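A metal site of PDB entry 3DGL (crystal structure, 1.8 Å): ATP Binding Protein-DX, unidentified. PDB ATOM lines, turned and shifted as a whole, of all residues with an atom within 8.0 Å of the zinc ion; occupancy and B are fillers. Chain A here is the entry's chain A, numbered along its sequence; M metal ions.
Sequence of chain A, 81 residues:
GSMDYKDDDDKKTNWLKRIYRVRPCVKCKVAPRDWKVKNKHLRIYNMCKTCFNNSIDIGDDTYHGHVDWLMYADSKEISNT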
ATOM      1  N   PRO A  24      30.662 -10.840 -25.240  1.00  0.00           N
ATOM      2  CA  PRO A  24      30.457 -12.248 -24.934  1.00  0.00           C
ATOM      3  C   PRO A  24      28.978 -12.634 -25.060  1.00  0.00           C
ATOM      4  O   PRO A  24      28.134 -11.806 -25.422  1.00  0.00           O
ATOM      5  CB  PRO A  24      30.895 -12.351 -23.471  1.00  0.00           C
ATOM      6  CG  PRO A  24      30.572 -11.022 -22.909  1.00  0.00           C
ATOM      7  CD  PRO A  24      30.871 -10.036 -24.013  1.00  0.00           C
ATOM      8  N   CYS A  25      28.703 -13.902 -24.756  1.00  0.00           N
ATOM      9  CA  CYS A  25      27.366 -14.461 -24.757  1.00  0.00           C
ATOM     10  C   CYS A  25      26.344 -13.489 -24.137  1.00  0.00           C
ATOM     11  O   CYS A  25      26.585 -12.970 -23.047  1.00  0.00           O
ATOM     12  CB  CYS A  25      27.402 -15.765 -23.947  1.00  0.00           C
ATOM     13  SG  CYS A  25      25.784 -16.522 -23.740  1.00  0.00           S
ATOM     14  N   VAL A  26      25.218 -13.270 -24.824  1.00  0.00           N
ATOM     15  CA  VAL A  26      24.189 -12.341 -24.325  1.00  0.00           C
ATOM     16  C   VAL A  26      23.477 -12.847 -23.051  1.00  0.00           C
ATOM     17  O   VAL A  26      22.814 -12.076 -22.347  1.00  0.00           O
ATOM     18  CB  VAL A  26      23.108 -12.032 -25.418  1.00  0.00           C
ATOM     19  CG1 VAL A  26      23.735 -11.345 -26.633  1.00  0.00           C
ATOM     20  CG2 VAL A  26      22.346 -13.292 -25.800  1.00  0.00           C
ATOM     21  N   LYS A  27      23.612 -14.142 -22.764  1.00  0.00           N
ATOM     22  CA  LYS A  27      22.904 -14.762 -21.643  1.00  0.00           C
ATOM     23  C   LYS A  27      23.785 -14.842 -20.385  1.00  0.00           C
ATOM     24  O   LYS A  27      23.421 -14.308 -19.339  1.00  0.00           O
ATOM     25  CB  LYS A  27      22.358 -16.159 -22.034  1.00  0.00           C
ATOM     26  CG  LYS A  27      21.552 -16.880 -20.912  1.00  0.00           C
ATOM     27  CD  LYS A  27      20.228 -16.157 -20.620  1.00  0.00           C
ATOM     28  CE  LYS A  27      19.528 -16.734 -19.378  1.00  0.00           C
ATOM     29  NZ  LYS A  27      18.313 -15.930 -19.078  1.00  0.00           N
ATOM     30  N   CYS A  28      24.934 -15.510 -20.473  1.00  0.00           N
ATOM     31  CA  CYS A  28      25.799 -15.641 -19.301  1.00  0.00           C
ATOM     32  C   CYS A  28      26.757 -14.455 -19.144  1.00  0.00           C
ATOM     33  O   CYS A  28      27.313 -14.223 -18.062  1.00  0.00           O
ATOM     34  CB  CYS A  28      26.589 -16.960 -19.325  1.00  0.00           C
ATOM     35  SG  CYS A  28      27.842 -17.069 -20.635  1.00  0.00           S
ATOM     36  N   LYS A  29      26.938 -13.728 -20.246  1.00  0.00           N
ATOM     37  CA  LYS A  29      27.755 -12.496 -20.287  1.00  0.00           C
ATOM     38  C   LYS A  29      29.238 -12.731 -19.966  1.00  0.00           C
ATOM     39  O   LYS A  29      29.947 -11.796 -19.612  1.00  0.00           O
ATOM     40  CB  LYS A  29      27.113 -11.391 -19.437  1.00  0.00           C
ATOM     41  CG  LYS A  29      25.736 -11.004 -19.991  1.00  0.00           C
ATOM     42  CD  LYS A  29      24.848 -10.304 -18.997  1.00  0.00           C
ATOM     43  CE  LYS A  29      23.520 -10.000 -19.680  1.00  0.00           C
ATOM     44  NZ  LYS A  29      22.763  -8.923 -18.988  1.00  0.00           N
ATOM     45  N   VAL A  30      29.697 -13.975 -20.127  1.00  0.00           N
ATOM     46  CA  VAL A  30      31.078 -14.333 -19.808  1.00  0.00           C
ATOM     47  C   VAL A  30      31.743 -15.123 -20.939  1.00  0.00           C
ATOM     48  O   VAL A  30      32.809 -14.731 -21.443  1.00  0.00           O
ATOM     49  CB  VAL A  30      31.168 -15.128 -18.471  1.00  0.00           C
ATOM     50  CG1 VAL A  30      32.576 -15.695 -18.268  1.00  0.00           C
ATOM     51  CG2 VAL A  30      30.796 -14.236 -17.278  1.00  0.00           C
ATOM     52  N   ALA A  31      31.125 -16.242 -21.330  1.00  0.00           N
ATOM     53  CA  ALA A  31      31.689 -17.115 -22.355  1.00  0.00           C
ATOM     54  C   ALA A  31      31.565 -16.444 -23.713  1.00  0.00           C
ATOM     55  O   ALA A  31      30.595 -15.701 -23.952  1.00  0.00           O
ATOM     56  CB  ALA A  31      30.961 -18.458 -22.385  1.00  0.00           C
ATOM     57  N   PRO A  32      32.518 -16.728 -24.613  1.00  0.00           N
ATOM     58  CA  PRO A  32      32.371 -16.247 -25.995  1.00  0.00           C
ATOM     59  C   PRO A  32      31.245 -16.953 -26.744  1.00  0.00           C
ATOM     60  O   PRO A  32      30.795 -18.034 -26.340  1.00  0.00           O
ATOM     61  CB  PRO A  32      33.734 -16.516 -26.633  1.00  0.00           C
ATOM     62  CG  PRO A  32      34.396 -17.524 -25.767  1.00  0.00           C
ATOM     63  CD  PRO A  32      33.745 -17.529 -24.412  1.00  0.00           C
ATOM     64  N   ARG A  33      30.790 -16.345 -27.842  1.00  0.00           N
ATOM     65  CA  ARG A  33      29.631 -16.832 -28.582  1.00  0.00           C
ATOM     66  C   ARG A  33      29.941 -18.014 -29.491  1.00  0.00           C
ATOM     67  O   ARG A  33      31.061 -18.140 -30.020  1.00  0.00           O
ATOM     68  CB  ARG A  33      29.049 -15.675 -29.395  1.00  0.00           C
ATOM     69  CG  ARG A  33      28.433 -14.619 -28.486  1.00  0.00           C
ATOM     70  CD  ARG A  33      28.060 -13.361 -29.265  1.00  0.00           C
ATOM     71  NE  ARG A  33      27.725 -12.274 -28.332  1.00  0.00           N
ATOM     72  CZ  ARG A  33      27.016 -11.200 -28.646  1.00  0.00           C
ATOM     73  NH1 ARG A  33      26.531 -11.032 -29.879  1.00  0.00           N
ATOM     74  NH2 ARG A  33      26.808 -10.267 -27.722  1.00  0.00           N
ATOM     75  N   ASP A  34      28.950 -18.876 -29.701  1.00  0.00           N
ATOM     76  CA  ASP A  34      29.087 -19.847 -30.775  1.00  0.00           C
ATOM     77  C   ASP A  34      29.101 -19.119 -32.128  1.00  0.00           C
ATOM     78  O   ASP A  34      28.660 -17.967 -32.236  1.00  0.00           O
ATOM     79  CB  ASP A  34      27.974 -20.900 -30.725  1.00  0.00           C
ATOM     80  CG  ASP A  34      28.294 -22.126 -31.593  1.00  0.00           C
ATOM     81  OD1 ASP A  34      29.487 -22.393 -31.875  1.00  0.00           O
ATOM     82  OD2 ASP A  34      27.342 -22.816 -31.990  1.00  0.00           O
ATOM     83  N   ASN A  46      24.132 -15.461 -30.912  1.00  0.00           N
ATOM     84  CA  ASN A  46      24.036 -14.549 -29.791  1.00  0.00           C
ATOM     85  C   ASN A  46      24.549 -15.158 -28.477  1.00  0.00           C
ATOM     86  O   ASN A  46      24.980 -14.418 -27.617  1.00  0.00           O
ATOM     87  CB  ASN A  46      22.615 -14.020 -29.607  1.00  0.00           C
ATOM     88  CG  ASN A  46      22.170 -13.163 -30.763  1.00  0.00           C
ATOM     89  OD1 ASN A  46      22.998 -12.671 -31.512  1.00  0.00           O
ATOM     90  ND2 ASN A  46      20.866 -12.959 -30.910  1.00  0.00           N
ATOM     91  N   MET A  47      24.485 -16.488 -28.368  1.00  0.00           N
ATOM     92  CA  MET A  47      24.894 -17.183 -27.131  1.00  0.00           C
ATOM     93  C   MET A  47      26.059 -18.141 -27.341  1.00  0.00           C
ATOM     94  O   MET A  47      26.327 -18.597 -28.469  1.00  0.00           O
ATOM     95  CB  MET A  47      23.720 -17.967 -26.524  1.00  0.00           C
ATOM     96  CG  MET A  47      22.667 -17.076 -25.841  1.00  0.00           C
ATOM     97  SD  MET A  47      21.303 -18.055 -25.100  1.00  0.00           S
ATOM     98  CE  MET A  47      20.474 -18.561 -26.600  1.00  0.00           C
ATOM     99  N   CYS A  48      26.736 -18.459 -26.235  1.00  0.00           N
ATOM    100  CA  CYS A  48      27.681 -19.575 -26.198  1.00  0.00           C
ATOM    101  C   CYS A  48      26.853 -20.867 -26.342  1.00  0.00           C
ATOM    102  O   CYS A  48      25.612 -20.836 -26.227  1.00  0.00           O
ATOM    103  CB  CYS A  48      28.502 -19.572 -24.899  1.00  0.00           C
ATOM    104  SG  CYS A  48      27.558 -20.030 -23.397  1.00  0.00           S
ATOM    105  N   LYS A  49      27.538 -21.991 -26.601  1.00  0.00           N
ATOM    106  CA  LYS A  49      26.828 -23.260 -26.811  1.00  0.00           C
ATOM    107  C   LYS A  49      26.117 -23.713 -25.523  1.00  0.00           C
ATOM    108  O   LYS A  49      24.990 -24.198 -25.563  1.00  0.00           O
ATOM    109  CB  LYS A  49      27.769 -24.359 -27.287  1.00  0.00           C
ATOM    110  CG  LYS A  49      26.998 -25.538 -27.901  1.00  0.00           C
ATOM    111  CD  LYS A  49      26.556 -25.200 -29.338  1.00  0.00           C
ATOM    112  CE  LYS A  49      25.592 -26.225 -29.885  1.00  0.00           C
ATOM    113  NZ  LYS A  49      25.108 -25.888 -31.260  1.00  0.00           N
ATOM    114  N   THR A  50      26.790 -23.544 -24.392  1.00  0.00           N
ATOM    115  CA  THR A  50      26.225 -23.934 -23.109  1.00  0.00           C
ATOM    116  C   THR A  50      24.871 -23.257 -22.882  1.00  0.00           C
ATOM    117  O   THR A  50      23.878 -23.934 -22.576  1.00  0.00           O
ATOM    118  CB  THR A  50      27.176 -23.597 -21.951  1.00  0.00           C
ATOM    119  OG1 THR A  50      28.427 -24.267 -22.170  1.00  0.00           O
ATOM    120  CG2 THR A  50      26.572 -24.053 -20.604  1.00  0.00           C
ATOM    121  N   CYS A  51      24.838 -21.951 -23.072  1.00  0.00           N
ATOM    122  CA  CYS A  51      23.592 -21.206 -22.836  1.00  0.00           C
ATOM    123  C   CYS A  51      22.548 -21.535 -23.898  1.00  0.00           C
ATOM    124  O   CYS A  51      21.362 -21.624 -23.594  1.00  0.00           O
ATOM    125  CB  CYS A  51      23.852 -19.691 -22.767  1.00  0.00           C
ATOM    126  SG  CYS A  51      24.720 -19.218 -21.238  1.00  0.00           S
ATOM    127  N   PHE A  52      22.992 -21.733 -25.135  1.00  0.00           N
ATOM    128  CA  PHE A  52      22.039 -22.098 -26.172  1.00  0.00           C
ATOM    129  C   PHE A  52      21.350 -23.452 -25.887  1.00  0.00           C
ATOM    130  O   PHE A  52      20.120 -23.569 -25.952  1.00  0.00           O
ATOM    131  CB  PHE A  52      22.707 -22.148 -27.549  1.00  0.00           C
ATOM    132  CG  PHE A  52      21.783 -22.649 -28.608  1.00  0.00           C
ATOM    133  CD1 PHE A  52      20.729 -21.848 -29.037  1.00  0.00           C
ATOM    134  CD2 PHE A  52      21.907 -23.947 -29.105  1.00  0.00           C
ATOM    135  CE1 PHE A  52      19.825 -22.310 -29.994  1.00  0.00           C
ATOM    136  CE2 PHE A  52      21.012 -24.424 -30.064  1.00  0.00           C
ATOM    137  CZ  PHE A  52      19.963 -23.613 -30.512  1.00  0.00           C
HETATM  138 ZN    ZN M   1      26.559 -18.215 -22.244  1.00  0.00          ZN
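Four residues have an atom within 4 Å of the zinc ion: Cys 25, Cys 28, Cys 48 and Cys 51.
The side-chain sulfur of Cys 28 lies close to the backbone NH of Ala 31, at 3.5 Å.
SG of Cys 28 sits close to N of Val 30 (3.6 Å).
The side-chain sulfur of Cys 48 sits close to the backbone NH of Thr 50, at 3.7 Å.
The backbone carbonyl oxygen of Ala 31 sits at hydrogen-bond distance from the backbone NH of Cys 25 (2.7 Å).
The side-chain sulfur (SG) of Cys 25 lies close to the backbone NH (N) of Lys 27 (3.4 Å).
The zinc ion is bound by the side-chain sulfur (SG) of Cys 51 (2.3 Å), the side-chain sulfur (SG) of Cys 28 (2.4 Å), the side-chain sulfur (SG) of Cys 48 (2.4 Å) and the side-chain sulfur (SG) of Cys 25 (2.4 Å).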
